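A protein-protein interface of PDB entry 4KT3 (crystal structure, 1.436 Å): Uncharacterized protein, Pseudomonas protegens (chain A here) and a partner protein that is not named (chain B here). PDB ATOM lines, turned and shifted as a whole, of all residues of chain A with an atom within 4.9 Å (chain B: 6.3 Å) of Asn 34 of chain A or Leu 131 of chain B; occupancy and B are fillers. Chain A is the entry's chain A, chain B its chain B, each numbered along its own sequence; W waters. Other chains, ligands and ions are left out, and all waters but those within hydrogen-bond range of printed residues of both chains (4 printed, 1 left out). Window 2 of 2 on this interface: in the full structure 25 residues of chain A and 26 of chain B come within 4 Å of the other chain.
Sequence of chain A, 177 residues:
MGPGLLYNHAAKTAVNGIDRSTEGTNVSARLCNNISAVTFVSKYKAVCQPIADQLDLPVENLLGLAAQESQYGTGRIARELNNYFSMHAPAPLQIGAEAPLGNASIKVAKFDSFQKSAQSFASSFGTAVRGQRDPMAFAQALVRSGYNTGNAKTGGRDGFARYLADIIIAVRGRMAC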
ATOM      1  N   ARG A  30       2.959  18.360 -22.438  1.00  0.00           N
ATOM      2  CA  ARG A  30       1.564  18.666 -22.740  1.00  0.00           C
ATOM      3  C   ARG A  30       1.457  19.908 -23.620  1.00  0.00           C
ATOM      4  O   ARG A  30       0.729  19.908 -24.617  1.00  0.00           O
ATOM      5  CB  ARG A  30       0.753  18.854 -21.453  1.00  0.00           C
ATOM      6  N   LEU A  31       2.184  20.961 -23.256  1.00  0.00           N
ATOM      7  CA  LEU A  31       2.140  22.209 -24.016  1.00  0.00           C
ATOM      8  C   LEU A  31       2.396  21.969 -25.494  1.00  0.00           C
ATOM      9  O   LEU A  31       1.758  22.603 -26.337  1.00  0.00           O
ATOM     10  CB  LEU A  31       3.159  23.227 -23.486  1.00  0.00           C
ATOM     11  CG  LEU A  31       2.786  23.942 -22.189  1.00  0.00           C
ATOM     12  CD1 LEU A  31       3.959  24.771 -21.679  1.00  0.00           C
ATOM     13  CD2 LEU A  31       1.549  24.816 -22.397  1.00  0.00           C
ATOM     14  N   CYS A  32       3.319  21.054 -25.805  1.00  0.00           N
ATOM     15  CA  CYS A  32       3.750  20.855 -27.193  1.00  0.00           C
ATOM     16  C   CYS A  32       2.743  20.053 -28.018  1.00  0.00           C
ATOM     17  O   CYS A  32       2.878  19.943 -29.238  1.00  0.00           O
ATOM     18  CB  CYS A  32       5.116  20.166 -27.243  1.00  0.00           C
ATOM     19  SG  CYS A  32       6.489  21.052 -26.439  1.00  0.00           S
ATOM     20  N   ASN A  33       1.730  19.500 -27.358  1.00  0.00           N
ATOM     21  CA  ASN A  33       0.737  18.683 -28.043  1.00  0.00           C
ATOM     22  C   ASN A  33      -0.370  19.501 -28.703  1.00  0.00           C
ATOM     23  O   ASN A  33      -1.113  18.984 -29.540  1.00  0.00           O
ATOM     24  CB  ASN A  33       0.128  17.672 -27.067  1.00  0.00           C
ATOM     25  CG  ASN A  33       1.118  16.627 -26.637  1.00  0.00           C
ATOM     26  OD1 ASN A  33       2.051  16.318 -27.368  1.00  0.00           O
ATOM     27  ND2 ASN A  33       0.923  16.074 -25.446  1.00  0.00           N
ATOM     28  N   ASN A  34      -0.476  20.777 -28.337  1.00  0.00           N
ATOM     29  CA  ASN A  34      -1.412  21.681 -28.987  1.00  0.00           C
ATOM     30  C   ASN A  34      -0.727  22.232 -30.230  1.00  0.00           C
ATOM     31  O   ASN A  34      -0.004  23.232 -30.174  1.00  0.00           O
ATOM     32  CB  ASN A  34      -1.797  22.807 -28.030  1.00  0.00           C
ATOM     33  CG  ASN A  34      -2.822  23.752 -28.616  1.00  0.00           C
ATOM     34  OD1 ASN A  34      -2.997  23.827 -29.839  1.00  0.00           O
ATOM     35  ND2 ASN A  34      -3.516  24.489 -27.738  1.00  0.00           N
ATOM     36  N   ILE A  35      -0.936  21.563 -31.353  1.00  0.00           N
ATOM     37  CA  ILE A  35      -0.172  21.880 -32.559  1.00  0.00           C
ATOM     38  C   ILE A  35      -0.470  23.298 -33.077  1.00  0.00           C
ATOM     39  O   ILE A  35       0.445  24.030 -33.483  1.00  0.00           O
ATOM     40  CB  ILE A  35      -0.406  20.812 -33.662  1.00  0.00           C
ATOM     41  CG1 ILE A  35      -0.031  19.405 -33.159  1.00  0.00           C
ATOM     42  CG2 ILE A  35       0.389  21.139 -34.899  1.00  0.00           C
ATOM     43  CD1 ILE A  35       1.351  19.288 -32.498  1.00  0.00           C
ATOM     44  N   SER A  36      -1.733  23.695 -33.044  1.00  0.00           N
ATOM     45  CA  SER A  36      -2.120  25.039 -33.468  1.00  0.00           C
ATOM     46  C   SER A  36      -1.319  26.076 -32.693  1.00  0.00           C
ATOM     47  O   SER A  36      -0.775  27.037 -33.277  1.00  0.00           O
ATOM     48  CB  SER A  36      -3.609  25.244 -33.214  1.00  0.00           C
ATOM     49  OG  SER A  36      -4.033  26.541 -33.592  1.00  0.00           O
ATOM     50  N   ALA A  37      -1.307  25.929 -31.371  1.00  0.00           N
ATOM     51  CA  ALA A  37      -0.607  26.902 -30.526  1.00  0.00           C
ATOM     52  C   ALA A  37       0.910  26.911 -30.779  1.00  0.00           C
ATOM     53  O   ALA A  37       1.529  27.975 -30.862  1.00  0.00           O
ATOM     54  CB  ALA A  37      -0.919  26.643 -29.054  1.00  0.00           C
ATOM     55  N   VAL A  38       1.512  25.735 -30.896  1.00  0.00           N
ATOM     56  CA  VAL A  38       2.949  25.638 -31.145  1.00  0.00           C
ATOM     57  C   VAL A  38       3.292  26.266 -32.491  1.00  0.00           C
ATOM     58  O   VAL A  38       4.278  26.975 -32.623  1.00  0.00           O
ATOM     59  CB  VAL A  38       3.435  24.156 -31.091  1.00  0.00           C
ATOM     60  CG1 VAL A  38       4.870  24.021 -31.617  1.00  0.00           C
ATOM     61  CG2 VAL A  38       3.348  23.623 -29.665  1.00  0.00           C
ATOM     62  N   ARG A 174       5.876  27.023 -24.791  1.00  0.00           N
ATOM     63  CA  ARG A 174       5.693  26.586 -26.169  1.00  0.00           C
ATOM     64  C   ARG A 174       6.827  27.032 -27.087  1.00  0.00           C
ATOM     65  O   ARG A 174       7.047  26.441 -28.146  1.00  0.00           O
ATOM     66  CB  ARG A 174       4.323  27.042 -26.695  1.00  0.00           C
ATOM     67  CG  ARG A 174       3.209  26.230 -26.068  1.00  0.00           C
ATOM     68  CD  ARG A 174       1.822  26.522 -26.591  1.00  0.00           C
ATOM     69  NE  ARG A 174       0.949  25.406 -26.176  1.00  0.00           N
ATOM     70  CZ  ARG A 174      -0.209  25.500 -25.526  1.00  0.00           C
ATOM     71  NH1 ARG A 174      -0.744  26.669 -25.203  1.00  0.00           N
ATOM     72  NH2 ARG A 174      -0.860  24.391 -25.206  1.00  0.00           N
ATOM     73  N   PRO B  58      -9.091  24.382 -35.827  1.00  0.00           N
ATOM     74  CA  PRO B  58      -7.706  24.256 -35.344  1.00  0.00           C
ATOM     75  C   PRO B  58      -7.403  23.004 -34.531  1.00  0.00           C
ATOM     76  O   PRO B  58      -6.234  22.599 -34.472  1.00  0.00           O
ATOM     77  CB  PRO B  58      -7.522  25.509 -34.476  1.00  0.00           C
ATOM     78  CG  PRO B  58      -8.497  26.507 -35.046  1.00  0.00           C
ATOM     79  CD  PRO B  58      -9.701  25.656 -35.401  1.00  0.00           C
ATOM     80  N   HIS B  59      -8.417  22.411 -33.901  1.00  0.00           N
ATOM     81  CA  HIS B  59      -8.213  21.241 -33.047  1.00  0.00           C
ATOM     82  C   HIS B  59      -9.095  20.102 -33.505  1.00  0.00           C
ATOM     83  O   HIS B  59     -10.295  20.114 -33.265  1.00  0.00           O
ATOM     84  CB  HIS B  59      -8.476  21.599 -31.585  1.00  0.00           C
ATOM     85  CG  HIS B  59      -7.478  22.581 -31.071  1.00  0.00           C
ATOM     86  ND1 HIS B  59      -7.712  23.940 -31.047  1.00  0.00           N
ATOM     87  CD2 HIS B  59      -6.201  22.407 -30.659  1.00  0.00           C
ATOM     88  CE1 HIS B  59      -6.630  24.560 -30.614  1.00  0.00           C
ATOM     89  NE2 HIS B  59      -5.695  23.652 -30.381  1.00  0.00           N
ATOM     90  N   PRO B  60      -8.493  19.147 -34.226  1.00  0.00           N
ATOM     91  CA  PRO B  60      -9.248  18.017 -34.776  1.00  0.00           C
ATOM     92  C   PRO B  60     -10.155  17.362 -33.738  1.00  0.00           C
ATOM     93  O   PRO B  60      -9.722  17.088 -32.614  1.00  0.00           O
ATOM     94  CB  PRO B  60      -8.143  17.064 -35.215  1.00  0.00           C
ATOM     95  CG  PRO B  60      -7.016  17.998 -35.625  1.00  0.00           C
ATOM     96  CD  PRO B  60      -7.077  19.131 -34.643  1.00  0.00           C
ATOM     97  N   TYR B  62     -12.889  18.851 -32.617  1.00  0.00           N
ATOM     98  CA  TYR B  62     -13.565  19.949 -31.919  1.00  0.00           C
ATOM     99  C   TYR B  62     -13.867  21.103 -32.876  1.00  0.00           C
ATOM    100  O   TYR B  62     -13.243  21.236 -33.938  1.00  0.00           O
ATOM    101  CB  TYR B  62     -12.672  20.497 -30.778  1.00  0.00           C
ATOM    102  CG  TYR B  62     -12.302  19.451 -29.762  1.00  0.00           C
ATOM    103  CD1 TYR B  62     -11.251  18.576 -29.996  1.00  0.00           C
ATOM    104  CD2 TYR B  62     -13.002  19.330 -28.576  1.00  0.00           C
ATOM    105  CE1 TYR B  62     -10.939  17.573 -29.090  1.00  0.00           C
ATOM    106  CE2 TYR B  62     -12.701  18.340 -27.662  1.00  0.00           C
ATOM    107  CZ  TYR B  62     -11.665  17.474 -27.913  1.00  0.00           C
ATOM    108  OH  TYR B  62     -11.360  16.481 -27.008  1.00  0.00           O
ATOM    109  N   ASP B  64     -13.710  25.278 -32.381  1.00  0.00           N
ATOM    110  CA  ASP B  64     -13.207  26.279 -31.439  1.00  0.00           C
ATOM    111  C   ASP B  64     -14.026  27.572 -31.500  1.00  0.00           C
ATOM    112  O   ASP B  64     -14.533  27.962 -32.567  1.00  0.00           O
ATOM    113  CB  ASP B  64     -11.746  26.625 -31.733  1.00  0.00           C
ATOM    114  CG  ASP B  64     -10.779  25.492 -31.438  1.00  0.00           C
ATOM    115  OD1 ASP B  64     -11.198  24.385 -31.037  1.00  0.00           O
ATOM    116  OD2 ASP B  64      -9.569  25.726 -31.650  1.00  0.00           O
ATOM    117  N   SER B  84     -12.976  24.835 -26.867  1.00  0.00           N
ATOM    118  CA  SER B  84     -13.087  23.754 -27.834  1.00  0.00           C
ATOM    119  C   SER B  84     -14.261  22.872 -27.421  1.00  0.00           C
ATOM    120  O   SER B  84     -14.343  22.443 -26.266  1.00  0.00           O
ATOM    121  CB  SER B  84     -11.797  22.926 -27.885  1.00  0.00           C
ATOM    122  OG  SER B  84     -10.692  23.694 -28.363  1.00  0.00           O
ATOM    123  N   TRP B  93     -13.994  22.457 -23.358  1.00  0.00           N
ATOM    124  CA  TRP B  93     -12.820  22.902 -22.622  1.00  0.00           C
ATOM    125  C   TRP B  93     -12.494  24.360 -22.907  1.00  0.00           C
ATOM    126  O   TRP B  93     -12.608  24.826 -24.038  1.00  0.00           O
ATOM    127  CB  TRP B  93     -11.595  22.072 -23.021  1.00  0.00           C
ATOM    128  CG  TRP B  93     -11.592  20.684 -22.478  1.00  0.00           C
ATOM    129  CD1 TRP B  93     -12.320  19.620 -22.935  1.00  0.00           C
ATOM    130  CD2 TRP B  93     -10.822  20.204 -21.377  1.00  0.00           C
ATOM    131  NE1 TRP B  93     -12.053  18.504 -22.180  1.00  0.00           N
ATOM    132  CE2 TRP B  93     -11.137  18.836 -21.213  1.00  0.00           C
ATOM    133  CE3 TRP B  93      -9.900  20.793 -20.511  1.00  0.00           C
ATOM    134  CZ2 TRP B  93     -10.554  18.053 -20.223  1.00  0.00           C
ATOM    135  CZ3 TRP B  93      -9.321  20.009 -19.529  1.00  0.00           C
ATOM    136  CH2 TRP B  93      -9.660  18.658 -19.387  1.00  0.00           C
ATOM    137  N   ILE B  95      -9.305  26.265 -23.329  1.00  0.00           N
ATOM    138  CA  ILE B  95      -8.014  25.659 -23.649  1.00  0.00           C
ATOM    139  C   ILE B  95      -6.788  26.544 -23.359  1.00  0.00           C
ATOM    140  O   ILE B  95      -5.651  26.163 -23.653  1.00  0.00           O
ATOM    141  CB  ILE B  95      -7.984  25.094 -25.093  1.00  0.00           C
ATOM    142  CG1 ILE B  95      -8.255  26.176 -26.147  1.00  0.00           C
ATOM    143  CG2 ILE B  95      -9.006  23.980 -25.231  1.00  0.00           C
ATOM    144  CD1 ILE B  95      -7.928  25.710 -27.568  1.00  0.00           C
ATOM    145  N   CYS B  98      -7.151  25.609 -19.454  1.00  0.00           N
ATOM    146  CA  CYS B  98      -7.232  24.150 -19.428  1.00  0.00           C
ATOM    147  C   CYS B  98      -8.216  23.631 -18.380  1.00  0.00           C
ATOM    148  O   CYS B  98      -7.884  22.797 -17.525  1.00  0.00           O
ATOM    149  CB  CYS B  98      -5.842  23.535 -19.269  1.00  0.00           C
ATOM    150  SG  CYS B  98      -4.873  23.631 -20.808  1.00  0.00           S
ATOM    151  N   SER B 126      -7.067  10.757 -27.960  1.00  0.00           N
ATOM    152  CA  SER B 126      -5.987  11.325 -28.768  1.00  0.00           C
ATOM    153  C   SER B 126      -6.285  12.756 -29.195  1.00  0.00           C
ATOM    154  O   SER B 126      -5.426  13.629 -29.111  1.00  0.00           O
ATOM    155  CB  SER B 126      -5.755  10.480 -30.018  1.00  0.00           C
ATOM    156  OG  SER B 126      -5.126   9.262 -29.686  1.00  0.00           O
ATOM    157  N   GLN B 127      -7.507  13.000 -29.646  1.00  0.00           N
ATOM    158  CA  GLN B 127      -7.872  14.342 -30.074  1.00  0.00           C
ATOM    159  C   GLN B 127      -7.869  15.268 -28.864  1.00  0.00           C
ATOM    160  O   GLN B 127      -7.450  16.420 -28.967  1.00  0.00           O
ATOM    161  CB  GLN B 127      -9.231  14.350 -30.782  1.00  0.00           C
ATOM    162  CG  GLN B 127      -9.220  13.698 -32.169  1.00  0.00           C
ATOM    163  CD  GLN B 127      -9.054  12.198 -32.115  1.00  0.00           C
ATOM    164  OE1 GLN B 127      -9.607  11.523 -31.246  1.00  0.00           O
ATOM    165  NE2 GLN B 127      -8.276  11.661 -33.052  1.00  0.00           N
ATOM    166  N   ARG B 128      -8.354  14.789 -27.723  1.00  0.00           N
ATOM    167  CA  ARG B 128      -8.361  15.613 -26.527  1.00  0.00           C
ATOM    168  C   ARG B 128      -6.934  15.976 -26.130  1.00  0.00           C
ATOM    169  O   ARG B 128      -6.664  17.117 -25.739  1.00  0.00           O
ATOM    170  CB  ARG B 128      -9.099  14.930 -25.357  1.00  0.00           C
ATOM    171  CG  ARG B 128      -9.188  15.799 -24.105  1.00  0.00           C
ATOM    172  CD  ARG B 128     -10.190  15.248 -23.090  1.00  0.00           C
ATOM    173  NE  ARG B 128      -9.923  13.847 -22.783  1.00  0.00           N
ATOM    174  CZ  ARG B 128     -10.627  12.811 -23.236  1.00  0.00           C
ATOM    175  NH1 ARG B 128     -11.686  12.980 -24.018  1.00  0.00           N
ATOM    176  NH2 ARG B 128     -10.263  11.582 -22.905  1.00  0.00           N
ATOM    177  N   GLU B 129      -6.016  15.021 -26.254  1.00  0.00           N
ATOM    178  CA  GLU B 129      -4.608  15.290 -25.955  1.00  0.00           C
ATOM    179  C   GLU B 129      -4.078  16.413 -26.833  1.00  0.00           C
ATOM    180  O   GLU B 129      -3.217  17.186 -26.408  1.00  0.00           O
ATOM    181  CB  GLU B 129      -3.761  14.028 -26.117  1.00  0.00           C
ATOM    182  CG  GLU B 129      -4.034  13.011 -25.007  1.00  0.00           C
ATOM    183  CD  GLU B 129      -3.428  11.642 -25.266  1.00  0.00           C
ATOM    184  OE1 GLU B 129      -2.791  11.455 -26.322  1.00  0.00           O
ATOM    185  OE2 GLU B 129      -3.603  10.752 -24.403  1.00  0.00           O
ATOM    186  N   GLY B 130      -4.620  16.507 -28.042  1.00  0.00           N
ATOM    187  CA  GLY B 130      -4.305  17.588 -28.961  1.00  0.00           C
ATOM    188  C   GLY B 130      -4.715  18.985 -28.512  1.00  0.00           C
ATOM    189  O   GLY B 130      -4.330  19.971 -29.163  1.00  0.00           O
ATOM    190  N   LEU B 131      -5.489  19.094 -27.430  1.00  0.00           N
ATOM    191  CA  LEU B 131      -5.777  20.405 -26.846  1.00  0.00           C
ATOM    192  C   LEU B 131      -4.626  20.892 -25.963  1.00  0.00           C
ATOM    193  O   LEU B 131      -4.566  22.059 -25.602  1.00  0.00           O
ATOM    194  CB  LEU B 131      -7.068  20.378 -26.018  1.00  0.00           C
ATOM    195  CG  LEU B 131      -8.326  19.877 -26.725  1.00  0.00           C
ATOM    196  CD1 LEU B 131      -9.518  19.911 -25.757  1.00  0.00           C
ATOM    197  CD2 LEU B 131      -8.602  20.700 -27.969  1.00  0.00           C
ATOM    198  N   GLY B 132      -3.713  19.991 -25.611  1.00  0.00           N
ATOM    199  CA  GLY B 132      -2.544  20.375 -24.832  1.00  0.00           C
ATOM    200  C   GLY B 132      -2.854  20.689 -23.378  1.00  0.00           C
ATOM    201  O   GLY B 132      -2.137  21.469 -22.741  1.00  0.00           O
ATOM    202  N   CYS B 133      -3.897  20.061 -22.845  1.00  0.00           N
ATOM    203  CA  CYS B 133      -4.384  20.365 -21.499  1.00  0.00           C
ATOM    204  C   CYS B 133      -4.304  19.193 -20.528  1.00  0.00           C
ATOM    205  O   CYS B 133      -4.567  19.356 -19.334  1.00  0.00           O
ATOM    206  CB  CYS B 133      -5.830  20.841 -21.569  1.00  0.00           C
ATOM    207  SG  CYS B 133      -6.019  22.528 -22.122  1.00  0.00           S
ATOM    208  N   GLU B 134      -3.968  18.013 -21.034  1.00  0.00           N
ATOM    209  CA  GLU B 134      -3.813  16.831 -20.189  1.00  0.00           C
ATOM    210  C   GLU B 134      -2.717  15.953 -20.787  1.00  0.00           C
ATOM    211  O   GLU B 134      -2.500  15.962 -21.997  1.00  0.00           O
ATOM    212  CB  GLU B 134      -5.137  16.058 -20.063  1.00  0.00           C
ATOM    213  CG  GLU B 134      -5.540  15.248 -21.302  1.00  0.00           C
ATOM    214  CD  GLU B 134      -6.917  14.597 -21.169  1.00  0.00           C
ATOM    215  OE1 GLU B 134      -7.072  13.424 -21.576  1.00  0.00           O
ATOM    216  OE2 GLU B 134      -7.846  15.256 -20.662  1.00  0.00           O
HETATM  217  O   HOH W   1      -3.325  19.819 -31.665  1.00  0.00           O
HETATM  218  O   HOH W   2      -2.543  26.620 -22.554  1.00  0.00           O
HETATM  219  O   HOH W   3      -3.821  24.401 -24.663  1.00  0.00           O
HETATM  220  O   HOH W   4      -3.955  21.789 -33.372  1.00  0.00           O
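Asn 34 of chain A touches just these residues of chain B: His 59 (2.8 Å), Gly 130 (3.4 Å) and Leu 131 (3.4 Å). Leu 131 of chain B touches just one residue of chain A: Asn 34. Of the printed residues of chain A, Pro 58 of chain B touches Ser 36. Printed residues of chain B within 4 Å of Ser 36 of chain A: Pro 58 (3.7 Å) and His 59 (3.9 Å). Of the printed residues of chain A, Gly 132 of chain B touches Arg 30. Printed residues of chain A within 4 Å of His 59 of chain B: Asn 34 (2.8 Å) and Ser 36 (3.9 Å). Ser 84 of chain B touches none of the printed residues of chain A. The nearest residue of chain B that does not touch Asn 34 of chain A is Gly 132 of chain B (4.1 Å). The nearest residue of chain A that does not touch Leu 131 of chain B is Arg 174 of chain A (4.4 Å).
The backbone NH of Ser 36 of chain A sits close to the side-chain amide oxygen of Asn 34 of chain A (3.4 Å). The side-chain amide oxygen (OD1) of Asn 34 of chain A sits at hydrogen-bond distance from the backbone NH (N) of Ala 37 of chain A, 3.1 Å away. The side-chain carboxylate (OD2) of Asp 64 of chain B lies within hydrogen-bond range of a ring nitrogen (ND1) of His 59 of chain B (2.6 Å). The side-chain sulfur (SG) of Cys 98 of chain B is disulfide-bonded to the side-chain sulfur (SG) of Cys 133 of chain B, at 2.1 Å.
Water W3 lies within hydrogen-bond range of O of Leu 131 of chain B (2.6 Å), O of Ile 95 of chain B (2.7 Å), NH2 of Arg 174 of chain A (3.0 Å) and ND2 of Asn 34 of chain A (3.1 Å). Water W4 lies within hydrogen-bond range of the backbone carbonyl oxygen of Pro 58 of chain B (2.7 Å) and the backbone NH of Ser 36 of chain A (2.9 Å). Water W1 lies within hydrogen-bond range of the backbone carbonyl oxygen (O) of Gly 130 of chain B, the backbone NH (N) of Ile 35 of chain A and the backbone carbonyl oxygen (O) of Asn 33 of chain A. Water W2 bridges NH1 of Arg 174 of chain A (3.2 Å) and O of Ile 95 of chain B (3.3 Å).
Of the 10 printed residues of chain A, 4 touch a printed residue of chain B. Printed residues of chain A that touch a printed residue of chain B: Arg 30, Asn 33, Asn 34 and Ser 36. Along chain A the printed residues that touch a printed residue of chain B span positions 30 to 36. Of the 18 printed residues of chain B, 6 touch a printed residue of chain A. Hydrophobic or aromatic side chains of chain B that line the printed part of chain A: Pro 58 and His 59. Among the printed residues, 8 pairs touch across the chains. Among the printed residues, no Asp or Glu carboxylate lies within 4 Å of a Lys or Arg side-chain nitrogen of the other chain.
A ring nitrogen (NE2) of His 59 of chain B sits at hydrogen-bond distance from the side-chain amide oxygen (OD1) of Asn 34 of chain A (2.8 Å). O of Leu 131 of chain B is in hydrogen-bond range of ND2 of Asn 34 of chain A (3.4 Å). O of Asn 33 of chain A sits close to O of Gly 130 of chain B, 3.4 Å away.
O of Arg 30 of chain A touches CA of Gly 132 of chain B, 3.3 Å away. CB of Asn 33 of chain A touches O of Glu 129 of chain B, at 3.4 Å. CA of Asn 34 of chain A touches O of Gly 130 of chain B (3.4 Å). Pro 58 of chain B touches Ser 36 of chain A. CB of Ser 36 of chain A touches NE2 of His 59 of chain B, 3.9 Å away.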
